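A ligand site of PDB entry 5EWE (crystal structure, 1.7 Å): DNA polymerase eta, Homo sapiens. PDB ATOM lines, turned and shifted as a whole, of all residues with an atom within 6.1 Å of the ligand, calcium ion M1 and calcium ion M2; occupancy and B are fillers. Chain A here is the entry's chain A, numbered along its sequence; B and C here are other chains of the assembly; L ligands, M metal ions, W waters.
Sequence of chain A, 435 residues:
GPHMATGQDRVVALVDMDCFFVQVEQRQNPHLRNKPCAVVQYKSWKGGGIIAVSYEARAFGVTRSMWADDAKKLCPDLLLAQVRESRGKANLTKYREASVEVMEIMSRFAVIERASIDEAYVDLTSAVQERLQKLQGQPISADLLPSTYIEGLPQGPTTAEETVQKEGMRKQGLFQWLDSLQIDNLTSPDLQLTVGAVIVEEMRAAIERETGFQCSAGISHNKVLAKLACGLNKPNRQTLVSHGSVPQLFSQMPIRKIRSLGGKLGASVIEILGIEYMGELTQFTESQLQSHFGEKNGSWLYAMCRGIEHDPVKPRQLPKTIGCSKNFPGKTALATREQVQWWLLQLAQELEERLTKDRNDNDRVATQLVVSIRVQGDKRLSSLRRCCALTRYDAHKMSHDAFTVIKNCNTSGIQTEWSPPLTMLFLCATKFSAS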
ATOM      1  N   ASP A  16      -2.682  -8.298  33.715  1.00  0.00           N
ATOM      2  CA  ASP A  16      -2.405  -7.592  32.466  1.00  0.00           C
ATOM      3  C   ASP A  16      -1.474  -8.467  31.638  1.00  0.00           C
ATOM      4  O   ASP A  16      -0.345  -8.718  32.057  1.00  0.00           O
ATOM      5  CB  ASP A  16      -1.774  -6.222  32.796  1.00  0.00           C
ATOM      6  CG  ASP A  16      -1.634  -5.307  31.612  1.00  0.00           C
ATOM      7  OD1 ASP A  16      -1.430  -5.790  30.505  1.00  0.00           O
ATOM      8  OD2 ASP A  16      -1.690  -4.064  31.796  1.00  0.00           O
ATOM      9  N   MET A  17      -1.917  -8.919  30.463  1.00  0.00           N
ATOM     10  CA  MET A  17      -1.052  -9.790  29.659  1.00  0.00           C
ATOM     11  C   MET A  17       0.159  -9.012  29.158  1.00  0.00           C
ATOM     12  O   MET A  17       0.049  -7.857  28.767  1.00  0.00           O
ATOM     13  CB  MET A  17      -1.826 -10.360  28.468  1.00  0.00           C
ATOM     14  CG  MET A  17      -3.130 -11.035  28.832  1.00  0.00           C
ATOM     15  SD  MET A  17      -2.960 -12.339  30.062  1.00  0.00           S
ATOM     16  CE  MET A  17      -1.935 -13.539  29.225  1.00  0.00           C
ATOM     17  N   ASP A  18       1.332  -9.650  29.183  1.00  0.00           N
ATOM     18  CA  ASP A  18       2.536  -8.995  28.676  1.00  0.00           C
ATOM     19  C   ASP A  18       2.531  -8.992  27.155  1.00  0.00           C
ATOM     20  O   ASP A  18       2.220 -10.027  26.552  1.00  0.00           O
ATOM     21  CB  ASP A  18       3.791  -9.704  29.184  1.00  0.00           C
ATOM     22  CG  ASP A  18       3.898  -9.685  30.702  1.00  0.00           C
ATOM     23  OD1 ASP A  18       3.547  -8.664  31.324  1.00  0.00           O
ATOM     24  OD2 ASP A  18       4.368 -10.690  31.265  1.00  0.00           O
ATOM     25  N   CYS A  19       2.920  -7.859  26.538  1.00  0.00           N
ATOM     26  CA  CYS A  19       2.944  -7.659  25.085  1.00  0.00           C
ATOM     27  C   CYS A  19       2.012  -8.609  24.334  1.00  0.00           C
ATOM     28  O   CYS A  19       2.462  -9.480  23.570  1.00  0.00           O
ATOM     29  CB  CYS A  19       4.377  -7.787  24.542  1.00  0.00           C
ATOM     30  SG  CYS A  19       5.313  -9.239  24.991  1.00  0.00           S
ATOM     31  N   PHE A  20       0.715  -8.438  24.553  1.00  0.00           N
ATOM     32  CA  PHE A  20      -0.256  -9.510  24.350  1.00  0.00           C
ATOM     33  C   PHE A  20      -0.283  -9.994  22.905  1.00  0.00           C
ATOM     34  O   PHE A  20      -0.176 -11.192  22.642  1.00  0.00           O
ATOM     35  CB  PHE A  20      -1.648  -9.058  24.788  1.00  0.00           C
ATOM     36  CG  PHE A  20      -2.700 -10.127  24.641  1.00  0.00           C
ATOM     37  CD1 PHE A  20      -2.465 -11.402  25.120  1.00  0.00           C
ATOM     38  CD2 PHE A  20      -3.899  -9.850  24.011  1.00  0.00           C
ATOM     39  CE1 PHE A  20      -3.437 -12.398  24.989  1.00  0.00           C
ATOM     40  CE2 PHE A  20      -4.871 -10.846  23.880  1.00  0.00           C
ATOM     41  CZ  PHE A  20      -4.631 -12.105  24.364  1.00  0.00           C
ATOM     42  N   PHE A  21      -0.436  -9.060  21.945  1.00  0.00           N
ATOM     43  CA  PHE A  21      -0.554  -9.498  20.556  1.00  0.00           C
ATOM     44  C   PHE A  21       0.724 -10.183  20.098  1.00  0.00           C
ATOM     45  O   PHE A  21       0.676 -11.094  19.255  1.00  0.00           O
ATOM     46  CB  PHE A  21      -0.866  -8.332  19.614  1.00  0.00           C
ATOM     47  CG  PHE A  21      -2.265  -7.797  19.685  1.00  0.00           C
ATOM     48  CD1 PHE A  21      -3.111  -8.073  20.738  1.00  0.00           C
ATOM     49  CD2 PHE A  21      -2.731  -6.997  18.649  1.00  0.00           C
ATOM     50  CE1 PHE A  21      -4.390  -7.536  20.780  1.00  0.00           C
ATOM     51  CE2 PHE A  21      -4.019  -6.492  18.679  1.00  0.00           C
ATOM     52  CZ  PHE A  21      -4.838  -6.750  19.746  1.00  0.00           C
ATOM     53  N   VAL A  22       1.874  -9.723  20.597  1.00  0.00           N
ATOM     54  CA  VAL A  22       3.143 -10.382  20.268  1.00  0.00           C
ATOM     55  C   VAL A  22       3.141 -11.828  20.780  1.00  0.00           C
ATOM     56  O   VAL A  22       3.529 -12.757  20.067  1.00  0.00           O
ATOM     57  CB  VAL A  22       4.312  -9.566  20.842  1.00  0.00           C
ATOM     58  CG1 VAL A  22       5.625 -10.379  20.834  1.00  0.00           C
ATOM     59  CG2 VAL A  22       4.483  -8.282  20.041  1.00  0.00           C
ATOM     60  N   ILE A  51       1.463  -1.933  16.587  1.00  0.00           N
ATOM     61  CA  ILE A  51       0.489  -1.970  17.665  1.00  0.00           C
ATOM     62  C   ILE A  51       1.042  -2.641  18.930  1.00  0.00           C
ATOM     63  O   ILE A  51       0.540  -2.362  20.031  1.00  0.00           O
ATOM     64  CB  ILE A  51      -0.830  -2.643  17.207  1.00  0.00           C
ATOM     65  CG1 ILE A  51      -1.848  -2.750  18.338  1.00  0.00           C
ATOM     66  CG2 ILE A  51      -0.566  -4.001  16.602  1.00  0.00           C
ATOM     67  CD1 ILE A  51      -3.168  -3.329  17.885  1.00  0.00           C
ATOM     68  N   ALA A  52       2.055  -3.500  18.800  1.00  0.00           N
ATOM     69  CA  ALA A  52       2.592  -4.204  19.970  1.00  0.00           C
ATOM     70  C   ALA A  52       4.051  -4.573  19.723  1.00  0.00           C
ATOM     71  O   ALA A  52       4.443  -4.849  18.598  1.00  0.00           O
ATOM     72  CB  ALA A  52       1.775  -5.473  20.291  1.00  0.00           C
ATOM     73  N   VAL A  53       4.850  -4.586  20.817  1.00  0.00           N
ATOM     74  CA  VAL A  53       6.311  -4.669  20.729  1.00  0.00           C
ATOM     75  C   VAL A  53       6.835  -5.644  21.779  1.00  0.00           C
ATOM     76  O   VAL A  53       6.521  -5.495  22.967  1.00  0.00           O
ATOM     77  CB  VAL A  53       6.955  -3.283  20.949  1.00  0.00           C
ATOM     78  CG1 VAL A  53       8.451  -3.336  20.663  1.00  0.00           C
ATOM     79  CG2 VAL A  53       6.267  -2.233  20.108  1.00  0.00           C
ATOM     80  N   TYR A  55       9.520  -7.377  24.372  1.00  0.00           N
ATOM     81  CA  TYR A  55      10.450  -6.697  25.272  1.00  0.00           C
ATOM     82  C   TYR A  55      11.860  -6.633  24.698  1.00  0.00           C
ATOM     83  O   TYR A  55      12.583  -5.648  24.922  1.00  0.00           O
ATOM     84  CB  TYR A  55      10.403  -7.342  26.675  1.00  0.00           C
ATOM     85  CG  TYR A  55       9.193  -6.857  27.456  1.00  0.00           C
ATOM     86  CD1 TYR A  55       7.924  -7.354  27.173  1.00  0.00           C
ATOM     87  CD2 TYR A  55       9.288  -5.856  28.416  1.00  0.00           C
ATOM     88  CE1 TYR A  55       6.787  -6.899  27.853  1.00  0.00           C
ATOM     89  CE2 TYR A  55       8.147  -5.390  29.103  1.00  0.00           C
ATOM     90  CZ  TYR A  55       6.910  -5.906  28.814  1.00  0.00           C
ATOM     91  OH  TYR A  55       5.754  -5.466  29.478  1.00  0.00           O
ATOM     92  N   ARG A  58      11.768  -3.580  22.532  1.00  0.00           N
ATOM     93  CA  ARG A  58      11.683  -2.331  23.290  1.00  0.00           C
ATOM     94  C   ARG A  58      13.065  -1.845  23.702  1.00  0.00           C
ATOM     95  O   ARG A  58      13.281  -0.633  23.856  1.00  0.00           O
ATOM     96  CB  ARG A  58      10.795  -2.494  24.522  1.00  0.00           C
ATOM     97  CG  ARG A  58       9.354  -2.855  24.182  1.00  0.00           C
ATOM     98  CD  ARG A  58       8.530  -3.069  25.434  1.00  0.00           C
ATOM     99  NE  ARG A  58       7.269  -3.740  25.096  1.00  0.00           N
ATOM    100  CZ  ARG A  58       6.203  -3.777  25.899  1.00  0.00           C
ATOM    101  NH1 ARG A  58       6.223  -3.161  27.089  1.00  0.00           N
ATOM    102  NH2 ARG A  58       5.108  -4.414  25.509  1.00  0.00           N
ATOM    103  N   ARG A  64       4.931   1.428  20.366  1.00  0.00           N
ATOM    104  CA  ARG A  64       3.623   1.491  19.731  1.00  0.00           C
ATOM    105  C   ARG A  64       3.457   2.810  18.986  1.00  0.00           C
ATOM    106  O   ARG A  64       4.063   3.828  19.323  1.00  0.00           O
ATOM    107  CB  ARG A  64       2.538   1.332  20.799  1.00  0.00           C
ATOM    108  CG  ARG A  64       1.133   1.129  20.308  1.00  0.00           C
ATOM    109  CD  ARG A  64       0.249   0.735  21.490  1.00  0.00           C
ATOM    110  NE  ARG A  64       0.445   1.639  22.638  1.00  0.00           N
ATOM    111  CZ  ARG A  64       0.388   1.248  23.908  1.00  0.00           C
ATOM    112  NH1 ARG A  64       0.184  -0.023  24.208  1.00  0.00           N
ATOM    113  NH2 ARG A  64       0.553   2.140  24.884  1.00  0.00           N
ATOM    114  N   LEU A  92      -9.345  -8.165  14.220  1.00  0.00           N
ATOM    115  CA  LEU A  92      -8.678  -8.534  15.454  1.00  0.00           C
ATOM    116  C   LEU A  92      -9.243  -9.808  16.092  1.00  0.00           C
ATOM    117  O   LEU A  92      -9.004 -10.053  17.279  1.00  0.00           O
ATOM    118  CB  LEU A  92      -8.740  -7.369  16.442  1.00  0.00           C
ATOM    119  CG  LEU A  92      -8.222  -6.025  15.913  1.00  0.00           C
ATOM    120  CD1 LEU A  92      -8.440  -4.907  16.915  1.00  0.00           C
ATOM    121  CD2 LEU A  92      -6.753  -6.143  15.563  1.00  0.00           C
ATOM    122  N   SER A 116     -10.300  -4.615  29.436  1.00  0.00           N
ATOM    123  CA  SER A 116      -9.821  -4.346  28.088  1.00  0.00           C
ATOM    124  C   SER A 116      -9.637  -5.704  27.427  1.00  0.00           C
ATOM    125  O   SER A 116      -9.931  -6.743  28.021  1.00  0.00           O
ATOM    126  CB  SER A 116      -8.519  -3.557  28.098  1.00  0.00           C
ATOM    127  OG  SER A 116      -7.441  -4.369  28.543  1.00  0.00           O
ATOM    128  N   ILE A 117      -9.087  -5.706  26.202  1.00  0.00           N
ATOM    129  CA  ILE A 117      -8.855  -6.980  25.535  1.00  0.00           C
ATOM    130  C   ILE A 117      -7.885  -7.858  26.340  1.00  0.00           C
ATOM    131  O   ILE A 117      -7.961  -9.090  26.265  1.00  0.00           O
ATOM    132  CB  ILE A 117      -8.365  -6.751  24.093  1.00  0.00           C
ATOM    133  CG1 ILE A 117      -8.457  -8.053  23.290  1.00  0.00           C
ATOM    134  CG2 ILE A 117      -6.957  -6.202  24.080  1.00  0.00           C
ATOM    135  CD1 ILE A 117      -8.374  -7.857  21.782  1.00  0.00           C
ATOM    136  N   ASP A 118      -7.000  -7.257  27.161  1.00  0.00           N
ATOM    137  CA  ASP A 118      -6.014  -8.117  27.814  1.00  0.00           C
ATOM    138  C   ASP A 118      -5.828  -7.816  29.299  1.00  0.00           C
ATOM    139  O   ASP A 118      -4.786  -8.150  29.862  1.00  0.00           O
ATOM    140  CB  ASP A 118      -4.664  -8.014  27.108  1.00  0.00           C
ATOM    141  CG  ASP A 118      -3.947  -6.726  27.434  1.00  0.00           C
ATOM    142  OD1 ASP A 118      -4.617  -5.703  27.640  1.00  0.00           O
ATOM    143  OD2 ASP A 118      -2.704  -6.741  27.498  1.00  0.00           O
ATOM    144  N   GLU A 119      -6.804  -7.174  29.946  1.00  0.00           N
ATOM    145  CA  GLU A 119      -6.740  -6.861  31.373  1.00  0.00           C
ATOM    146  C   GLU A 119      -8.044  -7.254  32.033  1.00  0.00           C
ATOM    147  O   GLU A 119      -9.113  -7.082  31.444  1.00  0.00           O
ATOM    148  CB  GLU A 119      -6.516  -5.350  31.630  1.00  0.00           C
ATOM    149  CG  GLU A 119      -5.144  -4.835  31.316  1.00  0.00           C
ATOM    150  CD  GLU A 119      -5.016  -3.367  31.664  1.00  0.00           C
ATOM    151  OE1 GLU A 119      -5.939  -2.843  32.330  1.00  0.00           O
ATOM    152  OE2 GLU A 119      -4.029  -2.737  31.262  1.00  0.00           O
ATOM    153  N   LYS A 227      -3.903  -1.683  39.745  1.00  0.00           N
ATOM    154  CA  LYS A 227      -3.437  -1.311  38.420  1.00  0.00           C
ATOM    155  C   LYS A 227      -2.052  -0.686  38.481  1.00  0.00           C
ATOM    156  O   LYS A 227      -1.163  -1.035  37.696  1.00  0.00           O
ATOM    157  CB  LYS A 227      -4.425  -0.336  37.766  1.00  0.00           C
ATOM    158  CG  LYS A 227      -3.965   0.214  36.465  1.00  0.00           C
ATOM    159  CD  LYS A 227      -3.866  -0.928  35.489  1.00  0.00           C
ATOM    160  CE  LYS A 227      -3.987  -0.450  34.072  1.00  0.00           C
ATOM    161  NZ  LYS A 227      -3.614   0.977  33.977  1.00  0.00           N
ATOM    162  N   LYS A 234       7.022  -5.260  35.507  1.00  0.00           N
ATOM    163  CA  LYS A 234       6.744  -5.997  34.266  1.00  0.00           C
ATOM    164  C   LYS A 234       8.060  -6.398  33.590  1.00  0.00           C
ATOM    165  O   LYS A 234       9.054  -5.692  33.728  1.00  0.00           O
ATOM    166  CB  LYS A 234       5.902  -5.142  33.313  1.00  0.00           C
ATOM    167  CG  LYS A 234       4.385  -5.244  33.447  1.00  0.00           C
ATOM    168  CD  LYS A 234       3.694  -4.662  32.175  1.00  0.00           C
ATOM    169  CE  LYS A 234       2.204  -5.052  32.024  1.00  0.00           C
ATOM    170  NZ  LYS A 234       1.967  -6.388  31.313  1.00  0.00           N
ATOM    171  N   PRO A 235       8.076  -7.509  32.840  1.00  0.00           N
ATOM    172  CA  PRO A 235       7.014  -8.492  32.586  1.00  0.00           C
ATOM    173  C   PRO A 235       7.122  -9.725  33.478  1.00  0.00           C
ATOM    174  O   PRO A 235       8.135  -9.908  34.157  1.00  0.00           O
ATOM    175  CB  PRO A 235       7.249  -8.868  31.125  1.00  0.00           C
ATOM    176  CG  PRO A 235       8.765  -8.844  31.013  1.00  0.00           C
ATOM    177  CD  PRO A 235       9.223  -7.722  31.925  1.00  0.00           C
ATOM    178  P    DT B   8      -4.226   2.461  30.019  1.00  0.00           P
ATOM    179  OP1  DT B   8      -3.425   1.942  31.151  1.00  0.00           O
ATOM    180  OP2  DT B   8      -3.599   3.381  29.040  1.00  0.00           O
ATOM    181  O5'  DT B   8      -4.753   1.186  29.218  1.00  0.00           O
ATOM    182  C5'  DT B   8      -5.696   0.322  29.808  1.00  0.00           C
ATOM    183  C4'  DT B   8      -6.079  -0.776  28.821  1.00  0.00           C
ATOM    184  O4'  DT B   8      -6.759  -0.178  27.690  1.00  0.00           O
ATOM    185  C3'  DT B   8      -4.898  -1.543  28.247  1.00  0.00           C
ATOM    186  O3'  DT B   8      -5.270  -2.903  28.084  1.00  0.00           O
ATOM    187  C2'  DT B   8      -4.645  -0.848  26.910  1.00  0.00           C
ATOM    188  C1'  DT B   8      -6.063  -0.455  26.491  1.00  0.00           C
ATOM    189  N1   DT B   8      -6.134   0.756  25.613  1.00  0.00           N
ATOM    190  C2   DT B   8      -6.822   0.666  24.416  1.00  0.00           C
ATOM    191  O2   DT B   8      -7.354  -0.357  24.033  1.00  0.00           O
ATOM    192  N3   DT B   8      -6.846   1.820  23.676  1.00  0.00           N
ATOM    193  C4   DT B   8      -6.284   3.036  24.013  1.00  0.00           C
ATOM    194  O4   DT B   8      -6.367   4.018  23.283  1.00  0.00           O
ATOM    195  C5   DT B   8      -5.585   3.066  25.278  1.00  0.00           C
ATOM    196  C7   DT B   8      -4.935   4.338  25.739  1.00  0.00           C
ATOM    197  C6   DT B   8      -5.545   1.943  26.008  1.00  0.00           C
ATOM    198  P    DT C   3       0.614  10.555  12.335  1.00  0.00           P
ATOM    199  OP1  DT C   3       0.319  12.005  12.426  1.00  0.00           O
ATOM    200  OP2  DT C   3       1.953  10.040  12.679  1.00  0.00           O
ATOM    201  O5'  DT C   3      -0.474   9.787  13.221  1.00  0.00           O
ATOM    202  C5'  DT C   3      -0.114   8.622  13.962  1.00  0.00           C
ATOM    203  C4'  DT C   3      -0.613   7.375  13.254  1.00  0.00           C
ATOM    204  O4'  DT C   3      -0.277   6.181  14.026  1.00  0.00           O
ATOM    205  C3'  DT C   3      -2.136   7.311  13.024  1.00  0.00           C
ATOM    206  O3'  DT C   3      -2.388   6.970  11.669  1.00  0.00           O
ATOM    207  C2'  DT C   3      -2.578   6.191  13.964  1.00  0.00           C
ATOM    208  C1'  DT C   3      -1.363   5.295  13.892  1.00  0.00           C
ATOM    209  N1   DT C   3      -1.299   4.218  14.951  1.00  0.00           N
ATOM    210  C2   DT C   3      -1.217   2.903  14.556  1.00  0.00           C
ATOM    211  O2   DT C   3      -1.164   2.553  13.381  1.00  0.00           O
ATOM    212  N3   DT C   3      -1.167   1.999  15.589  1.00  0.00           N
ATOM    213  C4   DT C   3      -1.224   2.273  16.942  1.00  0.00           C
ATOM    214  O4   DT C   3      -1.187   1.387  17.793  1.00  0.00           O
ATOM    215  C5   DT C   3      -1.323   3.673  17.294  1.00  0.00           C
ATOM    216  C7   DT C   3      -1.367   4.091  18.730  1.00  0.00           C
ATOM    217  C6   DT C   3      -1.354   4.570  16.283  1.00  0.00           C
ATOM    218  P    DG C   4      -3.886   6.897  11.106  1.00  0.00           P
ATOM    219  OP1  DG C   4      -3.754   6.744   9.641  1.00  0.00           O
ATOM    220  OP2  DG C   4      -4.683   7.980  11.711  1.00  0.00           O
ATOM    221  O5'  DG C   4      -4.467   5.517  11.681  1.00  0.00           O
ATOM    222  C5'  DG C   4      -3.947   4.282  11.233  1.00  0.00           C
ATOM    223  C4'  DG C   4      -4.663   3.121  11.912  1.00  0.00           C
ATOM    224  O4'  DG C   4      -4.312   3.111  13.327  1.00  0.00           O
ATOM    225  C3'  DG C   4      -6.187   3.185  11.875  1.00  0.00           C
ATOM    226  O3'  DG C   4      -6.673   1.867  11.811  1.00  0.00           O
ATOM    227  C2'  DG C   4      -6.523   3.808  13.233  1.00  0.00           C
ATOM    228  C1'  DG C   4      -5.498   3.088  14.083  1.00  0.00           C
ATOM    229  N9   DG C   4      -5.247   3.716  15.367  1.00  0.00           N
ATOM    230  C8   DG C   4      -5.127   5.055  15.637  1.00  0.00           C
ATOM    231  N7   DG C   4      -4.891   5.316  16.890  1.00  0.00           N
ATOM    232  C5   DG C   4      -4.858   4.063  17.491  1.00  0.00           C
ATOM    233  C6   DG C   4      -4.645   3.688  18.832  1.00  0.00           C
ATOM    234  O6   DG C   4      -4.419   4.413  19.799  1.00  0.00           O
ATOM    235  N1   DG C   4      -4.683   2.302  18.996  1.00  0.00           N
ATOM    236  C2   DG C   4      -4.918   1.398  17.986  1.00  0.00           C
ATOM    237  N2   DG C   4      -4.935   0.089  18.325  1.00  0.00           N
ATOM    238  N3   DG C   4      -5.106   1.736  16.727  1.00  0.00           N
ATOM    239  C4   DG C   4      -5.082   3.079  16.556  1.00  0.00           C
ATOM    240  P    DA C   5      -8.241   1.564  11.714  1.00  0.00           P
ATOM    241  OP1  DA C   5      -8.412   0.621  10.586  1.00  0.00           O
ATOM    242  OP2  DA C   5      -8.979   2.840  11.770  1.00  0.00           O
ATOM    243  O5'  DA C   5      -8.560   0.747  13.039  1.00  0.00           O
ATOM    244  C5'  DA C   5      -7.996  -0.551  13.241  1.00  0.00           C
ATOM    245  C4'  DA C   5      -8.613  -1.212  14.448  1.00  0.00           C
ATOM    246  O4'  DA C   5      -8.153  -0.555  15.658  1.00  0.00           O
ATOM    247  C3'  DA C   5     -10.143  -1.187  14.506  1.00  0.00           C
ATOM    248  O3'  DA C   5     -10.586  -2.431  14.981  1.00  0.00           O
ATOM    249  C2'  DA C   5     -10.436  -0.075  15.514  1.00  0.00           C
ATOM    250  C1'  DA C   5      -9.256  -0.226  16.464  1.00  0.00           C
ATOM    251  N9   DA C   5      -8.907   0.991  17.201  1.00  0.00           N
ATOM    252  C8   DA C   5      -8.758   2.242  16.703  1.00  0.00           C
ATOM    253  N7   DA C   5      -8.400   3.129  17.604  1.00  0.00           N
ATOM    254  C5   DA C   5      -8.289   2.384  18.765  1.00  0.00           C
ATOM    255  C6   DA C   5      -7.932   2.730  20.090  1.00  0.00           C
ATOM    256  N6   DA C   5      -7.629   3.973  20.458  1.00  0.00           N
ATOM    257  N1   DA C   5      -7.921   1.740  21.003  1.00  0.00           N
ATOM    258  C2   DA C   5      -8.238   0.499  20.625  1.00  0.00           C
ATOM    259  N3   DA C   5      -8.581   0.061  19.419  1.00  0.00           N
ATOM    260  C4   DA C   5      -8.581   1.063  18.532  1.00  0.00           C
HETATM  261  N1  LIG L   1      -4.339  -0.766  22.690  1.00  0.00           N
HETATM  262  C1  LIG L   1      -4.716   0.032  21.637  1.00  0.00           C
HETATM  263  N2  LIG L   1      -4.292   1.334  21.584  1.00  0.00           N
HETATM  264  C2  LIG L   1      -3.459   1.866  22.532  1.00  0.00           C
HETATM  265  C3  LIG L   1      -3.071   1.056  23.608  1.00  0.00           C
HETATM  266  C4  LIG L   1      -3.426  -0.291  23.607  1.00  0.00           C
HETATM  267  O1  LIG L   1      -5.446  -0.424  20.765  1.00  0.00           O
HETATM  268  N3  LIG L   1      -3.054   3.129  22.409  1.00  0.00           N
HETATM  269  C5  LIG L   1      -4.881  -2.141  22.761  1.00  0.00           C
HETATM  270  C6  LIG L   1      -4.148  -3.019  21.750  1.00  0.00           C
HETATM  271  O2  LIG L   1      -5.057  -3.975  21.259  1.00  0.00           O
HETATM  272  C7  LIG L   1      -3.112  -3.729  22.565  1.00  0.00           C
HETATM  273  C8  LIG L   1      -3.837  -3.884  23.887  1.00  0.00           C
HETATM  274  O3  LIG L   1      -4.586  -2.687  24.029  1.00  0.00           O
HETATM  275  O4  LIG L   1      -2.816  -4.980  21.991  1.00  0.00           O
HETATM  276  C9  LIG L   1      -2.912  -4.109  25.074  1.00  0.00           C
HETATM  277  O5  LIG L   1      -2.327  -2.866  25.370  1.00  0.00           O
HETATM  278  P1  LIG L   1      -1.127  -2.753  26.400  1.00  0.00           P
HETATM  279  O6  LIG L   1      -1.437  -3.594  27.606  1.00  0.00           O
HETATM  280  O7  LIG L   1      -0.907  -1.279  26.657  1.00  0.00           O
HETATM  281  O8  LIG L   1       0.171  -3.266  25.643  1.00  0.00           O
HETATM  282  P2  LIG L   1       0.881  -4.705  25.603  1.00  0.00           P
HETATM  283  O9  LIG L   1       0.039  -5.797  26.230  1.00  0.00           O
HETATM  284  O10 LIG L   1       1.293  -4.885  24.157  1.00  0.00           O
HETATM  285  O11 LIG L   1       2.228  -4.413  26.406  1.00  0.00           O
HETATM  286  P3  LIG L   1       2.544  -4.506  27.994  1.00  0.00           P
HETATM  287  O12 LIG L   1       1.250  -4.642  28.725  1.00  0.00           O
HETATM  288  O13 LIG L   1       3.484  -5.636  28.216  1.00  0.00           O
HETATM  289  O14 LIG L   1       3.231  -3.194  28.294  1.00  0.00           O
HETATM  290 CA    CA M   1      -0.787  -5.756  28.348  1.00  0.00          CA
HETATM  291 CA    CA M   2      -3.466  -3.872  29.106  1.00  0.00          CA
HETATM  292  O   HOH W   1      -1.412   4.775  23.914  1.00  0.00           O
HETATM  293  O   HOH W   2       3.435  -3.647  23.118  1.00  0.00           O
HETATM  294  O   HOH W   3      -0.514  -6.302  22.579  1.00  0.00           O
HETATM  295  O   HOH W   4       3.171  -0.997  26.919  1.00  0.00           O
HETATM  296  O   HOH W   5      -6.241  -3.023  19.032  1.00  0.00           O
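An oxygen (O1) of the ligand lies close to N1 of DA 5 of chain C (3.3 Å).
Asp 18 touches the ligand.
Phe 21 touches the ligand (CZ to O2, 3.2 Å).
CD1 of Ile 51 touches O2 of the ligand, at 3.9 Å.
CB of Ala 52 touches O10 of the ligand (3.9 Å).
Ile 117 touches the ligand.
Hydrophobic or aromatic side chains within 4 Å of the ligand: Phe 20, Phe 21, Ile 51, Ala 52, Tyr 55 and Ile 117.
17 residues have an atom within 4 Å of the ligand: Asp 16, Met 17, Asp 18, Cys 19, Phe 20, Phe 21, Ile 51, Ala 52, Tyr 55, Arg 58, Arg 64, Ile 117, Asp 118, Lys 234, DT 8 of chain B, DG 4 of chain C and DA 5 of chain C.
The nearest printed residue that does not touch the ligand is DT 3 of chain C (4.2 Å).
O14 of the ligand lies within salt-bridge range of NH1 of Arg 58 (3.2 Å).
NH1 of Arg 64 is in salt-bridge range of O7 of the ligand (3.0 Å).
The backbone NH (N) of Cys 19 is in hydrogen-bond range of an oxygen (O13) of the ligand (2.8 Å).
The side-chain amino group of Lys 234 lies within salt-bridge range of an oxygen (O13) of the ligand.
N3 of the ligand sits at hydrogen-bond distance from O6 of DG 4 of chain C.
O9 of the ligand sits close to N of Phe 20 (3.2 Å).
OH of Tyr 55 sits at hydrogen-bond distance from O13 of the ligand, 2.6 Å away.
Water W2 lies within hydrogen-bond range of O10 of the ligand (2.7 Å), N of Val 53 (2.9 Å) and NH2 of Arg 58 (3.0 Å).
Water W5 bridges O2 of the ligand (2.7 Å) and N2 of DG 4 of chain C (3.4 Å).
Water W3 lies within hydrogen-bond range of O4 of the ligand (2.7 Å), N of Phe 21 (2.8 Å) and N of Phe 20 (3.2 Å).
Water W1 lies within hydrogen-bond range of N3 of the ligand (2.8 Å) and NH2 of Arg 64 (3.4 Å).
Calcium ion M2 is bound by O3' of DT 8 of chain B (2.3 Å).
The side-chain carboxylate (OE2) of Glu 119 is bound to calcium ion M2.
Calcium ion M2 is bound by O6 of the ligand.
The side-chain carboxylate (OD1) of Asp 118 binds calcium ion M2, at 2.6 Å.
Calcium ion M2 has four donor atoms within binding distance.
Slightly farther from calcium ion M2 lies OD1 of Asp 16 (3.1 Å).
Within 4 Å of calcium ion M1: Asp 16, Met 17 and Asp 118.
The nearest printed residue that does not touch calcium ion M1 is Lys 234 (4.1 Å).
Calcium ion M1 is bound by the side-chain carboxylate of Asp 16 (2.3 Å), an oxygen (O9) of the ligand (2.3 Å), the backbone carbonyl oxygen of Met 17 (2.3 Å), the side-chain carboxylate of Asp 118 (2.3 Å), an oxygen (O12) of the ligand (2.4 Å) and an oxygen (O6) of the ligand (2.4 Å).
Calcium ion M1 has six donor atoms within binding distance.
O3' of DT 8 of chain B lies close to the side-chain hydroxyl of Ser 116.
The backbone carbonyl oxygen (O) of Asp 16 lies within hydrogen-bond range of the side-chain amino group (NZ) of Lys 234 (3.4 Å).
The side-chain carboxylate (OD1) of Asp 18 lies within salt-bridge range of the side-chain amino group (NZ) of Lys 234, 2.8 Å away.
The guanidinium group of Arg 58 sits close to the side-chain hydroxyl of Tyr 55 (3.4 Å).
O of Val 53 lies within hydrogen-bond range of NE of Arg 58 (2.9 Å).
The side-chain carboxylate (OD2) of Asp 16 lies close to the side-chain carboxylate (OE2) of Glu 119, at 2.7 Å.
The side-chain amino group of Lys 227 is in salt-bridge range of OP1 of DT 8 of chain B (3.0 Å).
N of Glu 119 is in hydrogen-bond range of OG of Ser 116, at 3.2 Å.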
